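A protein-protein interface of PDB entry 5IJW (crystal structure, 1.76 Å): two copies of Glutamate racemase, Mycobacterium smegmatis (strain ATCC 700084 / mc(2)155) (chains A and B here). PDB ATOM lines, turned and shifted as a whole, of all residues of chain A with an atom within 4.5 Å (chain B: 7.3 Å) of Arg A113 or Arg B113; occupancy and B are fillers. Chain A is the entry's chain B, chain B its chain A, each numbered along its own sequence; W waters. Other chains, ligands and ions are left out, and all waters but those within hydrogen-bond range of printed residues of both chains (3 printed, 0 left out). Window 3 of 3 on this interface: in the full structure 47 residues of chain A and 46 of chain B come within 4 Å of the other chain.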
ATOM      1  N   ALA A 110       9.924  -7.281  22.632  1.00  0.00           N
ATOM      2  CA  ALA A 110       9.920  -7.985  23.909  1.00  0.00           C
ATOM      3  C   ALA A 110      10.967  -9.089  23.943  1.00  0.00           C
ATOM      4  O   ALA A 110      11.496  -9.410  25.013  1.00  0.00           O
ATOM      5  CB  ALA A 110       8.529  -8.569  24.172  1.00  0.00           C
ATOM      6  N   ALA A 111      11.269  -9.694  22.797  1.00  0.00           N
ATOM      7  CA  ALA A 111      12.058 -10.921  22.798  1.00  0.00           C
ATOM      8  C   ALA A 111      13.557 -10.672  22.798  1.00  0.00           C
ATOM      9  O   ALA A 111      14.317 -11.571  23.185  1.00  0.00           O
ATOM     10  CB  ALA A 111      11.694 -11.794  21.589  1.00  0.00           C
ATOM     11  N   THR A 112      14.000  -9.483  22.391  1.00  0.00           N
ATOM     12  CA  THR A 112      15.432  -9.254  22.276  1.00  0.00           C
ATOM     13  C   THR A 112      16.070  -9.146  23.657  1.00  0.00           C
ATOM     14  O   THR A 112      15.457  -8.663  24.619  1.00  0.00           O
ATOM     15  CB  THR A 112      15.738  -7.999  21.445  1.00  0.00           C
ATOM     16  OG1 THR A 112      17.164  -7.849  21.349  1.00  0.00           O
ATOM     17  CG2 THR A 112      15.162  -6.726  22.078  1.00  0.00           C
ATOM     18  N   ARG A 113      17.303  -9.647  23.761  1.00  0.00           N
ATOM     19  CA  ARG A 113      18.094  -9.479  24.980  1.00  0.00           C
ATOM     20  C   ARG A 113      19.038  -8.292  24.887  1.00  0.00           C
ATOM     21  O   ARG A 113      19.142  -7.516  25.848  1.00  0.00           O
ATOM     22  CB  ARG A 113      18.912 -10.740  25.298  1.00  0.00           C
ATOM     23  CG  ARG A 113      18.102 -11.909  25.875  1.00  0.00           C
ATOM     24  CD  ARG A 113      17.310 -12.587  24.787  1.00  0.00           C
ATOM     25  NE  ARG A 113      18.167 -13.297  23.844  1.00  0.00           N
ATOM     26  CZ  ARG A 113      17.907 -13.423  22.544  1.00  0.00           C
ATOM     27  NH1 ARG A 113      16.823 -12.863  22.004  1.00  0.00           N
ATOM     28  NH2 ARG A 113      18.737 -14.102  21.778  1.00  0.00           N
ATOM     29  N   ASN A 114      19.729  -8.127  23.754  1.00  0.00           N
ATOM     30  CA  ASN A 114      20.696  -7.043  23.614  1.00  0.00           C
ATOM     31  C   ASN A 114      20.117  -5.806  22.936  1.00  0.00           C
ATOM     32  O   ASN A 114      20.827  -4.805  22.802  1.00  0.00           O
ATOM     33  CB  ASN A 114      21.966  -7.523  22.876  1.00  0.00           C
ATOM     34  CG  ASN A 114      21.732  -7.865  21.412  1.00  0.00           C
ATOM     35  OD1 ASN A 114      20.653  -7.660  20.870  1.00  0.00           O
ATOM     36  ND2 ASN A 114      22.773  -8.387  20.759  1.00  0.00           N
ATOM     37  N   GLY A 115      18.848  -5.836  22.535  1.00  0.00           N
ATOM     38  CA  GLY A 115      18.224  -4.688  21.907  1.00  0.00           C
ATOM     39  C   GLY A 115      18.609  -4.451  20.465  1.00  0.00           C
ATOM     40  O   GLY A 115      18.391  -3.353  19.948  1.00  0.00           O
ATOM     41  N   ASP A 182      20.322 -10.228  17.859  1.00  0.00           N
ATOM     42  CA  ASP A 182      19.995 -11.469  18.553  1.00  0.00           C
ATOM     43  C   ASP A 182      18.558 -11.901  18.320  1.00  0.00           C
ATOM     44  O   ASP A 182      18.112 -12.877  18.931  1.00  0.00           O
ATOM     45  CB  ASP A 182      20.293 -11.360  20.056  1.00  0.00           C
ATOM     46  CG  ASP A 182      19.295 -10.496  20.818  1.00  0.00           C
ATOM     47  OD1 ASP A 182      18.356  -9.919  20.221  1.00  0.00           O
ATOM     48  OD2 ASP A 182      19.490 -10.366  22.046  1.00  0.00           O
ATOM     49  N   THR A 183      17.838 -11.192  17.450  1.00  0.00           N
ATOM     50  CA  THR A 183      16.439 -11.433  17.134  1.00  0.00           C
ATOM     51  C   THR A 183      16.265 -11.111  15.658  1.00  0.00           C
ATOM     52  O   THR A 183      16.826 -10.125  15.179  1.00  0.00           O
ATOM     53  CB  THR A 183      15.535 -10.542  17.985  1.00  0.00           C
ATOM     54  OG1 THR A 183      15.849 -10.744  19.368  1.00  0.00           O
ATOM     55  CG2 THR A 183      14.062 -10.844  17.729  1.00  0.00           C
ATOM     56  N   ASN A 205      21.943 -18.309  19.181  1.00  0.00           N
ATOM     57  CA  ASN A 205      21.639 -17.163  20.022  1.00  0.00           C
ATOM     58  C   ASN A 205      20.727 -16.151  19.344  1.00  0.00           C
ATOM     59  O   ASN A 205      20.537 -15.052  19.882  1.00  0.00           O
ATOM     60  CB  ASN A 205      22.928 -16.471  20.475  1.00  0.00           C
ATOM     61  CG  ASN A 205      23.702 -17.295  21.493  1.00  0.00           C
ATOM     62  OD1 ASN A 205      23.147 -18.179  22.147  1.00  0.00           O
ATOM     63  ND2 ASN A 205      24.991 -16.998  21.635  1.00  0.00           N
ATOM     64  N   THR A 207      16.971 -15.287  18.021  1.00  0.00           N
ATOM     65  CA  THR A 207      15.564 -15.650  18.108  1.00  0.00           C
ATOM     66  C   THR A 207      14.853 -15.277  16.814  1.00  0.00           C
ATOM     67  O   THR A 207      14.733 -14.086  16.502  1.00  0.00           O
ATOM     68  CB  THR A 207      14.901 -14.919  19.275  1.00  0.00           C
ATOM     69  OG1 THR A 207      15.507 -15.326  20.508  1.00  0.00           O
ATOM     70  CG2 THR A 207      13.401 -15.212  19.307  1.00  0.00           C
ATOM     71  N   ARG B 107      16.812 -23.470  23.304  1.00  0.00           N
ATOM     72  CA  ARG B 107      16.251 -22.213  22.823  1.00  0.00           C
ATOM     73  C   ARG B 107      15.757 -21.345  23.975  1.00  0.00           C
ATOM     74  O   ARG B 107      15.979 -20.132  23.980  1.00  0.00           O
ATOM     75  CB  ARG B 107      15.112 -22.483  21.842  1.00  0.00           C
ATOM     76  CG  ARG B 107      14.527 -21.210  21.235  1.00  0.00           C
ATOM     77  CD  ARG B 107      15.257 -20.792  19.956  1.00  0.00           C
ATOM     78  NE  ARG B 107      16.464 -19.997  20.173  1.00  0.00           N
ATOM     79  CZ  ARG B 107      16.467 -18.687  20.401  1.00  0.00           C
ATOM     80  NH1 ARG B 107      15.319 -18.023  20.476  1.00  0.00           N
ATOM     81  NH2 ARG B 107      17.614 -18.042  20.569  1.00  0.00           N
ATOM     82  N   ALA B 108      15.073 -21.946  24.951  1.00  0.00           N
ATOM     83  CA  ALA B 108      14.526 -21.162  26.059  1.00  0.00           C
ATOM     84  C   ALA B 108      15.632 -20.497  26.871  1.00  0.00           C
ATOM     85  O   ALA B 108      15.478 -19.356  27.331  1.00  0.00           O
ATOM     86  CB  ALA B 108      13.658 -22.047  26.959  1.00  0.00           C
ATOM     87  N   VAL B 109      16.759 -21.194  27.052  1.00  0.00           N
ATOM     88  CA  VAL B 109      17.895 -20.609  27.770  1.00  0.00           C
ATOM     89  C   VAL B 109      18.428 -19.388  27.032  1.00  0.00           C
ATOM     90  O   VAL B 109      18.777 -18.369  27.645  1.00  0.00           O
ATOM     91  CB  VAL B 109      18.995 -21.667  27.977  1.00  0.00           C
ATOM     92  CG1 VAL B 109      20.294 -21.018  28.523  1.00  0.00           C
ATOM     93  CG2 VAL B 109      18.494 -22.757  28.922  1.00  0.00           C
ATOM     94  N   ALA B 110      18.511 -19.473  25.707  1.00  0.00           N
ATOM     95  CA  ALA B 110      18.930 -18.321  24.922  1.00  0.00           C
ATOM     96  C   ALA B 110      17.877 -17.219  24.931  1.00  0.00           C
ATOM     97  O   ALA B 110      18.226 -16.034  24.876  1.00  0.00           O
ATOM     98  CB  ALA B 110      19.238 -18.748  23.487  1.00  0.00           C
ATOM     99  N   ALA B 111      16.594 -17.580  25.035  1.00  0.00           N
ATOM    100  CA  ALA B 111      15.519 -16.616  24.835  1.00  0.00           C
ATOM    101  C   ALA B 111      15.181 -15.786  26.070  1.00  0.00           C
ATOM    102  O   ALA B 111      14.598 -14.700  25.925  1.00  0.00           O
ATOM    103  CB  ALA B 111      14.254 -17.342  24.364  1.00  0.00           C
ATOM    104  N   THR B 112      15.491 -16.264  27.273  1.00  0.00           N
ATOM    105  CA  THR B 112      15.030 -15.565  28.461  1.00  0.00           C
ATOM    106  C   THR B 112      15.808 -14.268  28.673  1.00  0.00           C
ATOM    107  O   THR B 112      17.018 -14.186  28.422  1.00  0.00           O
ATOM    108  CB  THR B 112      15.122 -16.465  29.701  1.00  0.00           C
ATOM    109  OG1 THR B 112      14.612 -15.760  30.838  1.00  0.00           O
ATOM    110  CG2 THR B 112      16.560 -16.893  29.985  1.00  0.00           C
ATOM    111  N   ARG B 113      15.094 -13.232  29.103  1.00  0.00           N
ATOM    112  CA  ARG B 113      15.722 -11.973  29.467  1.00  0.00           C
ATOM    113  C   ARG B 113      15.974 -11.864  30.964  1.00  0.00           C
ATOM    114  O   ARG B 113      17.009 -11.330  31.370  1.00  0.00           O
ATOM    115  CB  ARG B 113      14.864 -10.787  28.999  1.00  0.00           C
ATOM    116  CG  ARG B 113      14.956 -10.514  27.493  1.00  0.00           C
ATOM    117  CD  ARG B 113      14.086 -11.430  26.634  1.00  0.00           C
ATOM    118  NE  ARG B 113      12.655 -11.247  26.878  1.00  0.00           N
ATOM    119  CZ  ARG B 113      11.784 -12.224  27.136  1.00  0.00           C
ATOM    120  NH1 ARG B 113      10.508 -11.927  27.335  1.00  0.00           N
ATOM    121  NH2 ARG B 113      12.170 -13.494  27.209  1.00  0.00           N
ATOM    122  N   ASN B 114      15.064 -12.374  31.796  1.00  0.00           N
ATOM    123  CA  ASN B 114      15.217 -12.262  33.241  1.00  0.00           C
ATOM    124  C   ASN B 114      15.683 -13.557  33.891  1.00  0.00           C
ATOM    125  O   ASN B 114      15.847 -13.595  35.111  1.00  0.00           O
ATOM    126  CB  ASN B 114      13.906 -11.772  33.886  1.00  0.00           C
ATOM    127  CG  ASN B 114      12.793 -12.808  33.847  1.00  0.00           C
ATOM    128  OD1 ASN B 114      12.944 -13.887  33.279  1.00  0.00           O
ATOM    129  ND2 ASN B 114      11.673 -12.487  34.486  1.00  0.00           N
ATOM    130  N   GLY B 115      15.908 -14.611  33.109  1.00  0.00           N
ATOM    131  CA  GLY B 115      16.449 -15.843  33.653  1.00  0.00           C
ATOM    132  C   GLY B 115      15.444 -16.724  34.347  1.00  0.00           C
ATOM    133  O   GLY B 115      15.837 -17.639  35.079  1.00  0.00           O
ATOM    134  N   ARG B 116      14.159 -16.482  34.136  1.00  0.00           N
ATOM    135  CA  ARG B 116      13.089 -17.228  34.793  1.00  0.00           C
ATOM    136  C   ARG B 116      12.256 -17.881  33.700  1.00  0.00           C
ATOM    137  O   ARG B 116      11.618 -17.182  32.905  1.00  0.00           O
ATOM    138  CB  ARG B 116      12.268 -16.304  35.684  1.00  0.00           C
ATOM    139  CG  ARG B 116      13.136 -15.651  36.761  1.00  0.00           C
ATOM    140  CD  ARG B 116      12.391 -14.607  37.568  1.00  0.00           C
ATOM    141  NE  ARG B 116      11.531 -15.220  38.567  1.00  0.00           N
ATOM    142  CZ  ARG B 116      11.964 -15.784  39.690  1.00  0.00           C
ATOM    143  NH1 ARG B 116      13.267 -15.826  39.965  1.00  0.00           N
ATOM    144  NH2 ARG B 116      11.089 -16.308  40.541  1.00  0.00           N
ATOM    145  N   ILE B 117      12.284 -19.216  33.655  1.00  0.00           N
ATOM    146  CA  ILE B 117      11.748 -20.002  32.547  1.00  0.00           C
ATOM    147  C   ILE B 117      10.688 -20.946  33.091  1.00  0.00           C
ATOM    148  O   ILE B 117      10.911 -21.613  34.108  1.00  0.00           O
ATOM    149  CB  ILE B 117      12.858 -20.800  31.835  1.00  0.00           C
ATOM    150  CG1 ILE B 117      13.935 -19.850  31.292  1.00  0.00           C
ATOM    151  CG2 ILE B 117      12.282 -21.666  30.730  1.00  0.00           C
ATOM    152  CD1 ILE B 117      15.169 -20.559  30.709  1.00  0.00           C
ATOM    153  N   VAL B 181       8.009 -15.745  35.267  1.00  0.00           N
ATOM    154  CA  VAL B 181       8.754 -16.251  34.117  1.00  0.00           C
ATOM    155  C   VAL B 181       8.512 -15.344  32.909  1.00  0.00           C
ATOM    156  O   VAL B 181       7.440 -14.744  32.758  1.00  0.00           O
ATOM    157  CB  VAL B 181       8.373 -17.706  33.788  1.00  0.00           C
ATOM    158  CG1 VAL B 181       8.544 -18.608  35.029  1.00  0.00           C
ATOM    159  CG2 VAL B 181       6.952 -17.786  33.229  1.00  0.00           C
ATOM    160  N   ASP B 182       9.516 -15.245  32.032  1.00  0.00           N
ATOM    161  CA  ASP B 182       9.344 -14.453  30.816  1.00  0.00           C
ATOM    162  C   ASP B 182       9.496 -15.305  29.565  1.00  0.00           C
ATOM    163  O   ASP B 182       9.515 -14.766  28.455  1.00  0.00           O
ATOM    164  CB  ASP B 182      10.309 -13.255  30.790  1.00  0.00           C
ATOM    165  CG  ASP B 182      11.763 -13.639  30.554  1.00  0.00           C
ATOM    166  OD1 ASP B 182      12.109 -14.842  30.470  1.00  0.00           O
ATOM    167  OD2 ASP B 182      12.583 -12.694  30.464  1.00  0.00           O
ATOM    168  N   THR B 183       9.559 -16.623  29.734  1.00  0.00           N
ATOM    169  CA  THR B 183       9.799 -17.595  28.681  1.00  0.00           C
ATOM    170  C   THR B 183       9.065 -18.853  29.097  1.00  0.00           C
ATOM    171  O   THR B 183       9.154 -19.249  30.262  1.00  0.00           O
ATOM    172  CB  THR B 183      11.300 -17.878  28.520  1.00  0.00           C
ATOM    173  OG1 THR B 183      11.993 -16.638  28.325  1.00  0.00           O
ATOM    174  CG2 THR B 183      11.562 -18.794  27.339  1.00  0.00           C
ATOM    175  N   LEU B 184       8.350 -19.475  28.162  1.00  0.00           N
ATOM    176  CA  LEU B 184       7.500 -20.615  28.486  1.00  0.00           C
ATOM    177  C   LEU B 184       7.640 -21.692  27.414  1.00  0.00           C
ATOM    178  O   LEU B 184       7.272 -21.471  26.255  1.00  0.00           O
ATOM    179  CB  LEU B 184       6.035 -20.175  28.638  1.00  0.00           C
ATOM    180  CG  LEU B 184       5.055 -21.306  28.950  1.00  0.00           C
ATOM    181  CD1 LEU B 184       5.482 -22.009  30.226  1.00  0.00           C
ATOM    182  CD2 LEU B 184       3.636 -20.780  29.075  1.00  0.00           C
ATOM    183  N   ASP B 204       1.934 -10.157  26.987  1.00  0.00           N
ATOM    184  CA  ASP B 204       2.699 -10.061  25.751  1.00  0.00           C
ATOM    185  C   ASP B 204       4.208 -10.097  25.969  1.00  0.00           C
ATOM    186  O   ASP B 204       4.942 -10.233  24.987  1.00  0.00           O
ATOM    187  CB  ASP B 204       2.296  -8.814  24.949  1.00  0.00           C
ATOM    188  CG  ASP B 204       2.265  -7.548  25.773  1.00  0.00           C
ATOM    189  OD1 ASP B 204       3.276  -7.221  26.428  1.00  0.00           O
ATOM    190  OD2 ASP B 204       1.217  -6.863  25.741  1.00  0.00           O
ATOM    191  N   ASN B 205       4.691 -10.063  27.213  1.00  0.00           N
ATOM    192  CA  ASN B 205       6.131 -10.133  27.418  1.00  0.00           C
ATOM    193  C   ASN B 205       6.679 -11.554  27.301  1.00  0.00           C
ATOM    194  O   ASN B 205       7.876 -11.721  27.062  1.00  0.00           O
ATOM    195  CB  ASN B 205       6.504  -9.554  28.787  1.00  0.00           C
ATOM    196  CG  ASN B 205       8.003  -9.411  28.972  1.00  0.00           C
ATOM    197  OD1 ASN B 205       8.666  -8.711  28.207  1.00  0.00           O
ATOM    198  ND2 ASN B 205       8.549 -10.078  29.985  1.00  0.00           N
ATOM    199  N   VAL B 206       5.852 -12.578  27.468  1.00  0.00           N
ATOM    200  CA  VAL B 206       6.358 -13.937  27.655  1.00  0.00           C
ATOM    201  C   VAL B 206       6.641 -14.564  26.294  1.00  0.00           C
ATOM    202  O   VAL B 206       5.769 -14.604  25.418  1.00  0.00           O
ATOM    203  CB  VAL B 206       5.378 -14.784  28.479  1.00  0.00           C
ATOM    204  CG1 VAL B 206       5.844 -16.242  28.541  1.00  0.00           C
ATOM    205  CG2 VAL B 206       5.270 -14.208  29.889  1.00  0.00           C
ATOM    206  N   THR B 207       7.876 -15.031  26.104  1.00  0.00           N
ATOM    207  CA  THR B 207       8.250 -15.727  24.880  1.00  0.00           C
ATOM    208  C   THR B 207       7.832 -17.185  24.980  1.00  0.00           C
ATOM    209  O   THR B 207       8.340 -17.902  25.844  1.00  0.00           O
ATOM    210  CB  THR B 207       9.760 -15.650  24.661  1.00  0.00           C
ATOM    211  OG1 THR B 207      10.152 -14.286  24.538  1.00  0.00           O
ATOM    212  CG2 THR B 207      10.169 -16.423  23.398  1.00  0.00           C
HETATM  213  O   HOH W   1      12.936 -13.990  23.950  1.00  0.00           O
HETATM  214  O   HOH W   2      20.872 -14.844  22.937  1.00  0.00           O
HETATM  215  O   HOH W   3      11.364  -8.970  28.143  1.00  0.00           O
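The guanidinium group of Arg A113 sits at hydrogen-bond distance from the backbone carbonyl oxygen of Ala B110, 2.9 Å away. The guanidinium group (NE) of Arg B113 is in hydrogen-bond range of the backbone carbonyl oxygen (O) of Ala A110 (2.9 Å). The guanidinium group of Arg B107 lies within hydrogen-bond range of the side-chain hydroxyl of Thr A207, 2.7 Å away.
NH2 of Arg A113 lies within hydrogen-bond range of O of Asn A205 (2.8 Å). OD1 of Asn B114 is in hydrogen-bond range of OG1 of Thr B112. The side-chain hydroxyl of Thr A112 lies within hydrogen-bond range of the side-chain carboxylate of Asp A182 (2.6 Å). The guanidinium group (NH2) of Arg B113 is in hydrogen-bond range of the side-chain hydroxyl (OG1) of Thr B183. The guanidinium group of Arg A113 lies within salt-bridge range of the side-chain carboxylate of Asp A182. NH2 of Arg B113 sits at hydrogen-bond distance from OG1 of Thr B207.
Ala A111 touches Arg B113. O of Thr A112 touches CG of Arg B113, 3.5 Å away. Arg A113 touches Ala B111 (CD to O, 3.6 Å). CG of Arg A113 touches O of Thr B112, 3.6 Å away. CG of Arg A113 touches CG of Arg B113 (3.8 Å). Asn A205 touches Arg B107 (C to NH2, 3.8 Å).
Printed residues of chain B within 4 Å of Ala A111: Arg B113. Arg A113 touches just these residues of chain B: Ala B110 (2.9 Å), Ala B111 (3.6 Å), Thr B112 (3.6 Å) and Arg B113 (3.8 Å). Of the printed residues of chain A, Thr B112 touches Arg A113. Of chain A, only Ala A110 (2.9 Å), Ala A111 (3.5 Å), Thr A112 (3.5 Å) and Arg A113 (3.8 Å) come within 4 Å of Arg B113. Asn B114 touches none of the printed residues of chain A. The nearest printed residue of chain A that does not touch Arg B113 is Asn A114 (6.5 Å). The nearest printed residue of chain A that does not touch Thr B112 is Ala A111 (6.3 Å).
Of the 10 printed residues of chain A, 6 touch a printed residue of chain B. Of the 19 printed residues of chain B, 5 touch a printed residue of chain A. Among the printed residues, no Asp or Glu carboxylate lies within 4 Å of a Lys or Arg side-chain nitrogen of the other chain.
Ala A110 touches Arg B113, and with the chains exchanged Arg A113 touches Ala B110. Ala A111 touches Arg B113, and with the chains exchanged Arg A113 touches Ala B111. Thr A112 touches Arg B113, and with the chains exchanged Arg A113 touches Thr B112. Arg A113 touches its own counterpart, Arg B113. Positions printed for both chains: 110, 111, 112, 113, 114, 115, 182, 183, 205 and 207. Of the 9 pairs that touch across the chains among the printed residues, 7 have their exchanged pair printed and touching as well.
Water W2 lies within hydrogen-bond range of NH2 of Arg A113 (2.5 Å), O of Asn A205 (3.1 Å) and O of Ala B110 (3.5 Å). Water W1 lies within hydrogen-bond range of O of Ala B111, OG1 of Thr B207, O of Ala A111 and NH2 of Arg B113. Water W3 lies within hydrogen-bond range of OD1 of Asn B205 (2.7 Å), NE of Arg B113 (2.9 Å) and O of Ala A110 (3.2 Å).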
